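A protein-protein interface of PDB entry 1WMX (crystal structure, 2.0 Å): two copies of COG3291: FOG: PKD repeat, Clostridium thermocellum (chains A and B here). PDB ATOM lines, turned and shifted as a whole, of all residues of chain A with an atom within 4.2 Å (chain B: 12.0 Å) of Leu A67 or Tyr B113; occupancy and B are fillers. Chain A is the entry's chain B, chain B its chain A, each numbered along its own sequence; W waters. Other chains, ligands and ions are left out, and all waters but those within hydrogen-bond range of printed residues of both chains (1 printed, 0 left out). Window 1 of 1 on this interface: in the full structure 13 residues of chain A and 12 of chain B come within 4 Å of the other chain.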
ATOM      1  N   GLY A  21      -9.385 -17.699   0.391  1.00  0.00           N
ATOM      2  CA  GLY A  21     -10.248 -17.213  -0.676  1.00  0.00           C
ATOM      3  C   GLY A  21     -11.228 -18.298  -1.085  1.00  0.00           C
ATOM      4  O   GLY A  21     -11.560 -19.170  -0.281  1.00  0.00           O
ATOM      5  N   TRP A  22     -11.695 -18.256  -2.330  1.00  0.00           N
ATOM      6  CA  TRP A  22     -12.633 -19.261  -2.814  1.00  0.00           C
ATOM      7  C   TRP A  22     -12.428 -19.471  -4.303  1.00  0.00           C
ATOM      8  O   TRP A  22     -12.402 -18.515  -5.063  1.00  0.00           O
ATOM      9  CB  TRP A  22     -14.084 -18.820  -2.570  1.00  0.00           C
ATOM     10  CG  TRP A  22     -15.110 -19.917  -2.781  1.00  0.00           C
ATOM     11  CD1 TRP A  22     -15.637 -20.756  -1.827  1.00  0.00           C
ATOM     12  CD2 TRP A  22     -15.700 -20.314  -4.029  1.00  0.00           C
ATOM     13  NE1 TRP A  22     -16.514 -21.649  -2.411  1.00  0.00           N
ATOM     14  CE2 TRP A  22     -16.571 -21.395  -3.760  1.00  0.00           C
ATOM     15  CE3 TRP A  22     -15.575 -19.858  -5.356  1.00  0.00           C
ATOM     16  CZ2 TRP A  22     -17.317 -22.030  -4.769  1.00  0.00           C
ATOM     17  CZ3 TRP A  22     -16.319 -20.493  -6.365  1.00  0.00           C
ATOM     18  CH2 TRP A  22     -17.176 -21.564  -6.060  1.00  0.00           C
ATOM     19  N   SER A  23     -12.277 -20.728  -4.696  1.00  0.00           N
ATOM     20  CA  SER A  23     -12.107 -21.110  -6.092  1.00  0.00           C
ATOM     21  C   SER A  23     -13.141 -22.199  -6.344  1.00  0.00           C
ATOM     22  O   SER A  23     -13.393 -23.029  -5.465  1.00  0.00           O
ATOM     23  CB  SER A  23     -10.703 -21.671  -6.337  1.00  0.00           C
ATOM     24  OG  SER A  23      -9.721 -20.660  -6.216  1.00  0.00           O
ATOM     25  N   ILE A  65     -13.956 -19.997 -11.393  1.00  0.00           N
ATOM     26  CA  ILE A  65     -13.376 -18.766 -10.897  1.00  0.00           C
ATOM     27  C   ILE A  65     -12.447 -19.037  -9.725  1.00  0.00           C
ATOM     28  O   ILE A  65     -12.606 -20.019  -9.013  1.00  0.00           O
ATOM     29  CB  ILE A  65     -14.487 -17.818 -10.432  1.00  0.00           C
ATOM     30  CG1 ILE A  65     -13.908 -16.450 -10.096  1.00  0.00           C
ATOM     31  CG2 ILE A  65     -15.195 -18.412  -9.215  1.00  0.00           C
ATOM     32  CD1 ILE A  65     -14.967 -15.427  -9.740  1.00  0.00           C
ATOM     33  N   SER A  66     -11.456 -18.172  -9.547  1.00  0.00           N
ATOM     34  CA  SER A  66     -10.543 -18.296  -8.423  1.00  0.00           C
ATOM     35  C   SER A  66     -10.392 -16.930  -7.774  1.00  0.00           C
ATOM     36  O   SER A  66      -9.956 -15.982  -8.429  1.00  0.00           O
ATOM     37  CB  SER A  66      -9.172 -18.795  -8.870  1.00  0.00           C
ATOM     38  OG  SER A  66      -8.300 -18.888  -7.752  1.00  0.00           O
ATOM     39  N   LEU A  67     -10.763 -16.820  -6.502  1.00  0.00           N
ATOM     40  CA  LEU A  67     -10.639 -15.558  -5.780  1.00  0.00           C
ATOM     41  C   LEU A  67      -9.541 -15.677  -4.725  1.00  0.00           C
ATOM     42  O   LEU A  67      -9.583 -16.553  -3.867  1.00  0.00           O
ATOM     43  CB  LEU A  67     -11.969 -15.180  -5.107  1.00  0.00           C
ATOM     44  CG  LEU A  67     -13.182 -14.962  -6.028  1.00  0.00           C
ATOM     45  CD1 LEU A  67     -14.457 -14.927  -5.211  1.00  0.00           C
ATOM     46  CD2 LEU A  67     -13.019 -13.675  -6.811  1.00  0.00           C
ATOM     47  N   LEU A  68      -8.548 -14.799  -4.809  1.00  0.00           N
ATOM     48  CA  LEU A  68      -7.446 -14.790  -3.851  1.00  0.00           C
ATOM     49  C   LEU A  68      -7.509 -13.476  -3.069  1.00  0.00           C
ATOM     50  O   LEU A  68      -7.222 -12.408  -3.603  1.00  0.00           O
ATOM     51  CB  LEU A  68      -6.112 -14.917  -4.586  1.00  0.00           C
ATOM     52  CG  LEU A  68      -5.945 -16.146  -5.489  1.00  0.00           C
ATOM     53  CD1 LEU A  68      -4.644 -16.036  -6.258  1.00  0.00           C
ATOM     54  CD2 LEU A  68      -5.982 -17.426  -4.655  1.00  0.00           C
ATOM     55  N   THR A  69      -7.886 -13.558  -1.799  1.00  0.00           N
ATOM     56  CA  THR A  69      -8.020 -12.370  -0.976  1.00  0.00           C
ATOM     57  C   THR A  69      -6.692 -11.685  -0.651  1.00  0.00           C
ATOM     58  O   THR A  69      -5.639 -12.327  -0.582  1.00  0.00           O
ATOM     59  CB  THR A  69      -8.731 -12.693   0.355  1.00  0.00           C
ATOM     60  OG1 THR A  69      -7.932 -13.611   1.100  1.00  0.00           O
ATOM     61  CG2 THR A  69     -10.098 -13.331   0.111  1.00  0.00           C
ATOM     62  N   TRP A  73     -10.677 -11.273   2.934  1.00  0.00           N
ATOM     63  CA  TRP A  73     -12.017 -10.783   2.590  1.00  0.00           C
ATOM     64  C   TRP A  73     -12.333  -9.322   2.974  1.00  0.00           C
ATOM     65  O   TRP A  73     -13.340  -8.761   2.542  1.00  0.00           O
ATOM     66  CB  TRP A  73     -13.101 -11.733   3.122  1.00  0.00           C
ATOM     67  CG  TRP A  73     -13.063 -13.088   2.451  1.00  0.00           C
ATOM     68  CD1 TRP A  73     -12.713 -14.287   3.024  1.00  0.00           C
ATOM     69  CD2 TRP A  73     -13.355 -13.376   1.077  1.00  0.00           C
ATOM     70  NE1 TRP A  73     -12.770 -15.295   2.092  1.00  0.00           N
ATOM     71  CE2 TRP A  73     -13.161 -14.765   0.887  1.00  0.00           C
ATOM     72  CE3 TRP A  73     -13.758 -12.595  -0.016  1.00  0.00           C
ATOM     73  CZ2 TRP A  73     -13.356 -15.390  -0.352  1.00  0.00           C
ATOM     74  CZ3 TRP A  73     -13.952 -13.218  -1.250  1.00  0.00           C
ATOM     75  CH2 TRP A  73     -13.750 -14.600  -1.405  1.00  0.00           C
ATOM     76  N   ARG A 105     -11.385  -7.457  -7.820  1.00  0.00           N
ATOM     77  CA  ARG A 105     -12.780  -7.278  -7.385  1.00  0.00           C
ATOM     78  C   ARG A 105     -12.755  -6.420  -6.142  1.00  0.00           C
ATOM     79  O   ARG A 105     -11.851  -6.539  -5.311  1.00  0.00           O
ATOM     80  CB  ARG A 105     -13.321  -8.654  -7.104  1.00  0.00           C
ATOM     81  CG  ARG A 105     -14.772  -8.836  -6.709  1.00  0.00           C
ATOM     82  CD  ARG A 105     -14.824 -10.298  -6.379  1.00  0.00           C
ATOM     83  NE  ARG A 105     -16.071 -11.016  -6.367  1.00  0.00           N
ATOM     84  CZ  ARG A 105     -16.544 -11.772  -7.361  1.00  0.00           C
ATOM     85  NH1 ARG A 105     -15.928 -11.857  -8.556  1.00  0.00           N
ATOM     86  NH2 ARG A 105     -17.606 -12.550  -7.198  1.00  0.00           N
ATOM     87  N   LEU A 158      -8.098 -10.623  -5.829  1.00  0.00           N
ATOM     88  CA  LEU A 158      -7.543 -10.872  -7.145  1.00  0.00           C
ATOM     89  C   LEU A 158      -8.383 -11.972  -7.718  1.00  0.00           C
ATOM     90  O   LEU A 158      -8.918 -12.805  -6.948  1.00  0.00           O
ATOM     91  CB  LEU A 158      -6.066 -11.229  -6.976  1.00  0.00           C
ATOM     92  CG  LEU A 158      -5.463 -11.998  -8.144  1.00  0.00           C
ATOM     93  CD1 LEU A 158      -5.343 -11.167  -9.422  1.00  0.00           C
ATOM     94  CD2 LEU A 158      -4.049 -12.503  -7.841  1.00  0.00           C
ATOM     95  N   VAL A 159      -8.494 -11.952  -9.037  1.00  0.00           N
ATOM     96  CA  VAL A 159      -9.350 -12.922  -9.716  1.00  0.00           C
ATOM     97  C   VAL A 159      -8.685 -13.528 -10.955  1.00  0.00           C
ATOM     98  O   VAL A 159      -8.197 -12.827 -11.842  1.00  0.00           O
ATOM     99  CB  VAL A 159     -10.643 -12.214 -10.127  1.00  0.00           C
ATOM    100  CG1 VAL A 159     -11.820 -13.173 -10.274  1.00  0.00           C
ATOM    101  CG2 VAL A 159     -11.092 -11.155  -9.105  1.00  0.00           C
ATOM    102  N   ASP B 106     -30.175 -12.152  -6.090  1.00  0.00           N
ATOM    103  CA  ASP B 106     -30.316 -12.555  -4.702  1.00  0.00           C
ATOM    104  C   ASP B 106     -29.259 -11.843  -3.862  1.00  0.00           C
ATOM    105  O   ASP B 106     -28.455 -11.049  -4.375  1.00  0.00           O
ATOM    106  CB  ASP B 106     -30.201 -14.085  -4.539  1.00  0.00           C
ATOM    107  CG  ASP B 106     -28.772 -14.612  -4.705  1.00  0.00           C
ATOM    108  OD1 ASP B 106     -28.586 -15.845  -4.576  1.00  0.00           O
ATOM    109  OD2 ASP B 106     -27.840 -13.818  -4.961  1.00  0.00           O
ATOM    110  N   LYS B 107     -29.272 -12.130  -2.569  1.00  0.00           N
ATOM    111  CA  LYS B 107     -28.337 -11.524  -1.631  1.00  0.00           C
ATOM    112  C   LYS B 107     -28.077 -12.527  -0.499  1.00  0.00           C
ATOM    113  O   LYS B 107     -29.004 -12.910   0.221  1.00  0.00           O
ATOM    114  CB  LYS B 107     -28.959 -10.251  -1.070  1.00  0.00           C
ATOM    115  CG  LYS B 107     -28.067  -9.403  -0.187  1.00  0.00           C
ATOM    116  CD  LYS B 107     -28.955  -8.538   0.681  1.00  0.00           C
ATOM    117  CE  LYS B 107     -28.394  -7.157   0.906  1.00  0.00           C
ATOM    118  NZ  LYS B 107     -29.362  -6.349   1.706  1.00  0.00           N
ATOM    119  N   VAL B 108     -26.830 -12.963  -0.363  1.00  0.00           N
ATOM    120  CA  VAL B 108     -26.444 -13.919   0.681  1.00  0.00           C
ATOM    121  C   VAL B 108     -25.094 -13.462   1.218  1.00  0.00           C
ATOM    122  O   VAL B 108     -24.059 -13.707   0.599  1.00  0.00           O
ATOM    123  CB  VAL B 108     -26.321 -15.361   0.114  1.00  0.00           C
ATOM    124  CG1 VAL B 108     -25.945 -16.348   1.226  1.00  0.00           C
ATOM    125  CG2 VAL B 108     -27.632 -15.775  -0.537  1.00  0.00           C
ATOM    126  N   TYR B 109     -25.110 -12.798   2.368  1.00  0.00           N
ATOM    127  CA  TYR B 109     -23.887 -12.262   2.963  1.00  0.00           C
ATOM    128  C   TYR B 109     -22.763 -13.231   3.277  1.00  0.00           C
ATOM    129  O   TYR B 109     -21.593 -12.855   3.229  1.00  0.00           O
ATOM    130  CB  TYR B 109     -24.225 -11.462   4.222  1.00  0.00           C
ATOM    131  CG  TYR B 109     -24.815 -10.102   3.919  1.00  0.00           C
ATOM    132  CD1 TYR B 109     -24.137  -9.199   3.096  1.00  0.00           C
ATOM    133  CD2 TYR B 109     -26.056  -9.724   4.436  1.00  0.00           C
ATOM    134  CE1 TYR B 109     -24.677  -7.960   2.792  1.00  0.00           C
ATOM    135  CE2 TYR B 109     -26.607  -8.482   4.141  1.00  0.00           C
ATOM    136  CZ  TYR B 109     -25.911  -7.607   3.316  1.00  0.00           C
ATOM    137  OH  TYR B 109     -26.444  -6.378   3.009  1.00  0.00           O
ATOM    138  N   GLU B 110     -23.130 -14.470   3.571  1.00  0.00           N
ATOM    139  CA  GLU B 110     -22.100 -15.376   3.992  1.00  0.00           C
ATOM    140  C   GLU B 110     -21.489 -16.152   2.751  1.00  0.00           C
ATOM    141  O   GLU B 110     -20.466 -16.866   2.865  1.00  0.00           O
ATOM    142  CB  GLU B 110     -22.669 -16.417   5.051  1.00  0.00           C
ATOM    143  CG  GLU B 110     -23.991 -16.292   5.925  1.00  0.00           C
ATOM    144  CD  GLU B 110     -25.150 -15.497   5.384  1.00  0.00           C
ATOM    145  OE1 GLU B 110     -25.071 -14.234   5.374  1.00  0.00           O
ATOM    146  OE2 GLU B 110     -26.199 -16.103   4.963  1.00  0.00           O
ATOM    147  N   ARG B 111     -22.039 -15.967   1.539  1.00  0.00           N
ATOM    148  CA  ARG B 111     -21.543 -16.615   0.320  1.00  0.00           C
ATOM    149  C   ARG B 111     -20.427 -15.731  -0.256  1.00  0.00           C
ATOM    150  O   ARG B 111     -20.662 -14.899  -1.133  1.00  0.00           O
ATOM    151  CB  ARG B 111     -22.691 -16.770  -0.678  1.00  0.00           C
ATOM    152  CG  ARG B 111     -22.424 -17.735  -1.816  1.00  0.00           C
ATOM    153  CD  ARG B 111     -23.611 -17.750  -2.738  1.00  0.00           C
ATOM    154  NE  ARG B 111     -24.002 -16.387  -3.098  1.00  0.00           N
ATOM    155  CZ  ARG B 111     -25.207 -16.044  -3.544  1.00  0.00           C
ATOM    156  NH1 ARG B 111     -26.150 -16.963  -3.691  1.00  0.00           N
ATOM    157  NH2 ARG B 111     -25.471 -14.780  -3.825  1.00  0.00           N
ATOM    158  N   VAL B 112     -19.209 -15.935   0.245  1.00  0.00           N
ATOM    159  CA  VAL B 112     -18.048 -15.123  -0.138  1.00  0.00           C
ATOM    160  C   VAL B 112     -17.645 -15.002  -1.605  1.00  0.00           C
ATOM    161  O   VAL B 112     -17.078 -13.985  -2.004  1.00  0.00           O
ATOM    162  CB  VAL B 112     -16.792 -15.528   0.684  1.00  0.00           C
ATOM    163  CG1 VAL B 112     -16.997 -15.170   2.142  1.00  0.00           C
ATOM    164  CG2 VAL B 112     -16.517 -17.009   0.544  1.00  0.00           C
ATOM    165  N   TYR B 113     -17.931 -16.009  -2.415  1.00  0.00           N
ATOM    166  CA  TYR B 113     -17.565 -15.932  -3.819  1.00  0.00           C
ATOM    167  C   TYR B 113     -18.512 -15.072  -4.672  1.00  0.00           C
ATOM    168  O   TYR B 113     -18.363 -15.002  -5.889  1.00  0.00           O
ATOM    169  CB  TYR B 113     -17.423 -17.349  -4.401  1.00  0.00           C
ATOM    170  CG  TYR B 113     -18.659 -18.210  -4.334  1.00  0.00           C
ATOM    171  CD1 TYR B 113     -19.592 -18.202  -5.365  1.00  0.00           C
ATOM    172  CD2 TYR B 113     -18.896 -19.047  -3.236  1.00  0.00           C
ATOM    173  CE1 TYR B 113     -20.728 -18.998  -5.310  1.00  0.00           C
ATOM    174  CE2 TYR B 113     -20.032 -19.846  -3.173  1.00  0.00           C
ATOM    175  CZ  TYR B 113     -20.941 -19.816  -4.212  1.00  0.00           C
ATOM    176  OH  TYR B 113     -22.071 -20.593  -4.150  1.00  0.00           O
ATOM    177  N   GLY B 114     -19.466 -14.403  -4.027  1.00  0.00           N
ATOM    178  CA  GLY B 114     -20.392 -13.538  -4.742  1.00  0.00           C
ATOM    179  C   GLY B 114     -21.614 -13.223  -3.903  1.00  0.00           C
ATOM    180  O   GLY B 114     -22.566 -14.000  -3.898  1.00  0.00           O
ATOM    181  N   LEU B 115     -21.589 -12.098  -3.188  1.00  0.00           N
ATOM    182  CA  LEU B 115     -22.700 -11.714  -2.315  1.00  0.00           C
ATOM    183  C   LEU B 115     -24.049 -11.604  -3.011  1.00  0.00           C
ATOM    184  O   LEU B 115     -25.085 -11.833  -2.397  1.00  0.00           O
ATOM    185  CB  LEU B 115     -22.407 -10.397  -1.597  1.00  0.00           C
ATOM    186  CG  LEU B 115     -21.324 -10.349  -0.512  1.00  0.00           C
ATOM    187  CD1 LEU B 115     -21.211 -11.660   0.251  1.00  0.00           C
ATOM    188  CD2 LEU B 115     -20.031 -10.063  -1.169  1.00  0.00           C
ATOM    189  N   GLU B 116     -24.036 -11.229  -4.281  1.00  0.00           N
ATOM    190  CA  GLU B 116     -25.261 -11.119  -5.055  1.00  0.00           C
ATOM    191  C   GLU B 116     -25.046 -11.840  -6.383  1.00  0.00           C
ATOM    192  O   GLU B 116     -24.032 -11.640  -7.044  1.00  0.00           O
ATOM    193  CB  GLU B 116     -25.608  -9.661  -5.330  1.00  0.00           C
ATOM    194  CG  GLU B 116     -25.653  -8.795  -4.102  1.00  0.00           C
ATOM    195  CD  GLU B 116     -25.875  -7.342  -4.442  1.00  0.00           C
ATOM    196  OE1 GLU B 116     -27.033  -6.886  -4.352  1.00  0.00           O
ATOM    197  OE2 GLU B 116     -24.895  -6.661  -4.811  1.00  0.00           O
ATOM    198  N   ILE B 117     -26.000 -12.684  -6.760  1.00  0.00           N
ATOM    199  CA  ILE B 117     -25.911 -13.425  -8.012  1.00  0.00           C
ATOM    200  C   ILE B 117     -27.168 -13.179  -8.840  1.00  0.00           C
ATOM    201  O   ILE B 117     -28.263 -13.124  -8.298  1.00  0.00           O
ATOM    202  CB  ILE B 117     -25.770 -14.950  -7.761  1.00  0.00           C
ATOM    203  CG1 ILE B 117     -24.495 -15.236  -6.968  1.00  0.00           C
ATOM    204  CG2 ILE B 117     -25.753 -15.700  -9.091  1.00  0.00           C
ATOM    205  CD1 ILE B 117     -24.302 -16.701  -6.642  1.00  0.00           C
ATOM    206  N   ASP B 118     -27.000 -13.031 -10.150  1.00  0.00           N
ATOM    207  CA  ASP B 118     -28.122 -12.796 -11.052  1.00  0.00           C
ATOM    208  C   ASP B 118     -28.376 -14.013 -11.939  1.00  0.00           C
ATOM    209  O   ASP B 118     -27.435 -14.608 -12.448  1.00  0.00           O
ATOM    210  CB  ASP B 118     -27.831 -11.595 -11.965  1.00  0.00           C
ATOM    211  CG  ASP B 118     -27.988 -10.244 -11.261  1.00  0.00           C
ATOM    212  OD1 ASP B 118     -27.527  -9.226 -11.824  1.00  0.00           O
ATOM    213  OD2 ASP B 118     -28.583 -10.192 -10.165  1.00  0.00           O
ATOM    214  N   VAL B 119     -29.641 -14.394 -12.094  1.00  0.00           N
ATOM    215  CA  VAL B 119     -30.020 -15.491 -12.987  1.00  0.00           C
ATOM    216  C   VAL B 119     -30.889 -14.775 -14.022  1.00  0.00           C
ATOM    217  O   VAL B 119     -31.907 -14.171 -13.676  1.00  0.00           O
ATOM    218  CB  VAL B 119     -30.828 -16.608 -12.267  1.00  0.00           C
ATOM    219  CG1 VAL B 119     -29.898 -17.426 -11.390  1.00  0.00           C
ATOM    220  CG2 VAL B 119     -31.942 -16.011 -11.427  1.00  0.00           C
ATOM    221  N   ILE B 146     -29.952 -23.806 -10.979  1.00  0.00           N
ATOM    222  CA  ILE B 146     -28.530 -23.929 -11.301  1.00  0.00           C
ATOM    223  C   ILE B 146     -27.569 -24.249 -10.162  1.00  0.00           C
ATOM    224  O   ILE B 146     -27.860 -24.042  -8.984  1.00  0.00           O
ATOM    225  CB  ILE B 146     -27.971 -22.651 -11.954  1.00  0.00           C
ATOM    226  CG1 ILE B 146     -28.864 -22.185 -13.091  1.00  0.00           C
ATOM    227  CG2 ILE B 146     -26.583 -22.926 -12.517  1.00  0.00           C
ATOM    228  CD1 ILE B 146     -28.279 -21.003 -13.835  1.00  0.00           C
ATOM    229  N   ASN B 147     -26.404 -24.743 -10.564  1.00  0.00           N
ATOM    230  CA  ASN B 147     -25.295 -25.089  -9.685  1.00  0.00           C
ATOM    231  C   ASN B 147     -24.474 -23.802  -9.632  1.00  0.00           C
ATOM    232  O   ASN B 147     -23.244 -23.826  -9.643  1.00  0.00           O
ATOM    233  CB  ASN B 147     -24.463 -26.177 -10.350  1.00  0.00           C
ATOM    234  CG  ASN B 147     -24.119 -25.828 -11.792  1.00  0.00           C
ATOM    235  OD1 ASN B 147     -23.514 -24.789 -12.065  1.00  0.00           O
ATOM    236  ND2 ASN B 147     -24.515 -26.690 -12.721  1.00  0.00           N
ATOM    237  N   ASN B 148     -25.177 -22.681  -9.592  1.00  0.00           N
ATOM    238  CA  ASN B 148     -24.552 -21.372  -9.585  1.00  0.00           C
ATOM    239  C   ASN B 148     -24.222 -20.879  -8.189  1.00  0.00           C
ATOM    240  O   ASN B 148     -23.242 -20.160  -7.982  1.00  0.00           O
ATOM    241  CB  ASN B 148     -25.501 -20.374 -10.240  1.00  0.00           C
ATOM    242  CG  ASN B 148     -24.776 -19.245 -10.906  1.00  0.00           C
ATOM    243  OD1 ASN B 148     -25.395 -18.358 -11.483  1.00  0.00           O
ATOM    244  ND2 ASN B 148     -23.453 -19.272 -10.843  1.00  0.00           N
ATOM    245  N   GLY B 149     -25.045 -21.281  -7.233  1.00  0.00           N
ATOM    246  CA  GLY B 149     -24.873 -20.825  -5.873  1.00  0.00           C
ATOM    247  C   GLY B 149     -26.035 -19.879  -5.638  1.00  0.00           C
ATOM    248  O   GLY B 149     -26.282 -19.456  -4.521  1.00  0.00           O
ATOM    249  N   PHE B 150     -26.744 -19.548  -6.718  1.00  0.00           N
ATOM    250  CA  PHE B 150     -27.907 -18.670  -6.646  1.00  0.00           C
ATOM    251  C   PHE B 150     -28.872 -19.303  -5.648  1.00  0.00           C
ATOM    252  O   PHE B 150     -29.140 -20.509  -5.714  1.00  0.00           O
ATOM    253  CB  PHE B 150     -28.592 -18.561  -8.009  1.00  0.00           C
ATOM    254  CG  PHE B 150     -29.819 -17.682  -8.008  1.00  0.00           C
ATOM    255  CD1 PHE B 150     -29.708 -16.296  -8.102  1.00  0.00           C
ATOM    256  CD2 PHE B 150     -31.092 -18.241  -7.884  1.00  0.00           C
ATOM    257  CE1 PHE B 150     -30.839 -15.474  -8.077  1.00  0.00           C
ATOM    258  CE2 PHE B 150     -32.232 -17.429  -7.856  1.00  0.00           C
ATOM    259  CZ  PHE B 150     -32.099 -16.037  -7.952  1.00  0.00           C
ATOM    260  N   ASP B 151     -29.389 -18.493  -4.732  1.00  0.00           N
ATOM    261  CA  ASP B 151     -30.317 -18.978  -3.721  1.00  0.00           C
ATOM    262  C   ASP B 151     -31.724 -18.391  -3.901  1.00  0.00           C
ATOM    263  O   ASP B 151     -31.976 -17.228  -3.579  1.00  0.00           O
ATOM    264  CB  ASP B 151     -29.773 -18.643  -2.333  1.00  0.00           C
ATOM    265  CG  ASP B 151     -30.680 -19.119  -1.234  1.00  0.00           C
ATOM    266  OD1 ASP B 151     -31.605 -19.891  -1.538  1.00  0.00           O
ATOM    267  OD2 ASP B 151     -30.461 -18.727  -0.066  1.00  0.00           O
ATOM    268  N   PRO B 152     -32.661 -19.203  -4.418  1.00  0.00           N
ATOM    269  CA  PRO B 152     -34.049 -18.776  -4.653  1.00  0.00           C
ATOM    270  C   PRO B 152     -34.839 -18.414  -3.402  1.00  0.00           C
ATOM    271  O   PRO B 152     -35.943 -17.870  -3.490  1.00  0.00           O
ATOM    272  CB  PRO B 152     -34.655 -19.956  -5.404  1.00  0.00           C
ATOM    273  CG  PRO B 152     -33.855 -21.124  -4.901  1.00  0.00           C
ATOM    274  CD  PRO B 152     -32.451 -20.588  -4.873  1.00  0.00           C
ATOM    275  N   SER B 154     -33.512 -16.448  -1.215  1.00  0.00           N
ATOM    276  CA  SER B 154     -32.900 -15.172  -0.831  1.00  0.00           C
ATOM    277  C   SER B 154     -32.966 -14.160  -1.973  1.00  0.00           C
ATOM    278  O   SER B 154     -32.033 -13.383  -2.179  1.00  0.00           O
ATOM    279  CB  SER B 154     -31.429 -15.379  -0.451  1.00  0.00           C
ATOM    280  OG  SER B 154     -31.277 -16.264   0.640  1.00  0.00           O
HETATM  281  O   HOH W   1     -16.783 -12.157  -3.994  1.00  0.00           O
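O of Tyr B113 sits at hydrogen-bond distance from NH2 of Arg A105, at 2.9 Å.
O of Gly B114 is in hydrogen-bond range of NE of Arg B111 (2.9 Å). O of Trp A22 sits at hydrogen-bond distance from N of Leu A67, 2.8 Å away.
Trp A22 touches Tyr B113 (CE3 to CB, 3.3 Å). Tyr B113 touches Leu A67 (CA to CD1, 3.6 Å). Trp A73 touches Val B112. Arg A105 touches Gly B114 (NH2 to CA, 3.8 Å).
Of chain B, only Tyr B113 (3.6 Å) comes within 4 Å of Leu A67. Of chain A, only Trp A22 (3.3 Å), Leu A67 (3.6 Å) and Arg A105 (2.9 Å) come within 4 Å of Tyr B113. Of chain B, only Tyr B113 comes within 4 Å of Trp A22. No residue of chain B comes within 4 Å of Ser A66. No residue of chain B comes within 4 Å of Leu A68. No residue of chain B comes within 4 Å of Thr A69. Arg A105 touches just these residues of chain B: Tyr B113 and Gly B114. Of the printed residues of chain B, Trp A73 touches Val B112 (3.3 Å). Of the printed residues of chain A, Gly B114 touches Arg A105 (3.8 Å). Asn B148 touches none of the printed residues of chain A. The nearest residue of chain B that does not touch Leu A67 is Val B112 (4.2 Å). The nearest printed residue of chain A that does not touch Tyr B113 is Trp A73 (4.5 Å).
Of the 22 printed residues of chain B, 3 touch a printed residue of chain A. Printed residues of chain B that touch a printed residue of chain A: Val B112, Tyr B113 and Gly B114. Printed residues of chain A that touch a printed residue of chain B: Trp A22, Leu A67, Trp A73 and Arg A105. Hydrophobic or aromatic side chains of chain A that line the printed part of chain B: Trp A22, Leu A67 and Trp A73.
No position is printed for both chains. Of the 5 pairs that touch across the chains among the printed residues, none has its exchanged pair printed and touching as well.
Water W1 lies within hydrogen-bond range of the backbone carbonyl oxygen (O) of Val B112, the guanidinium group (NE) of Arg A105 and the backbone NH (N) of Gly B114.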
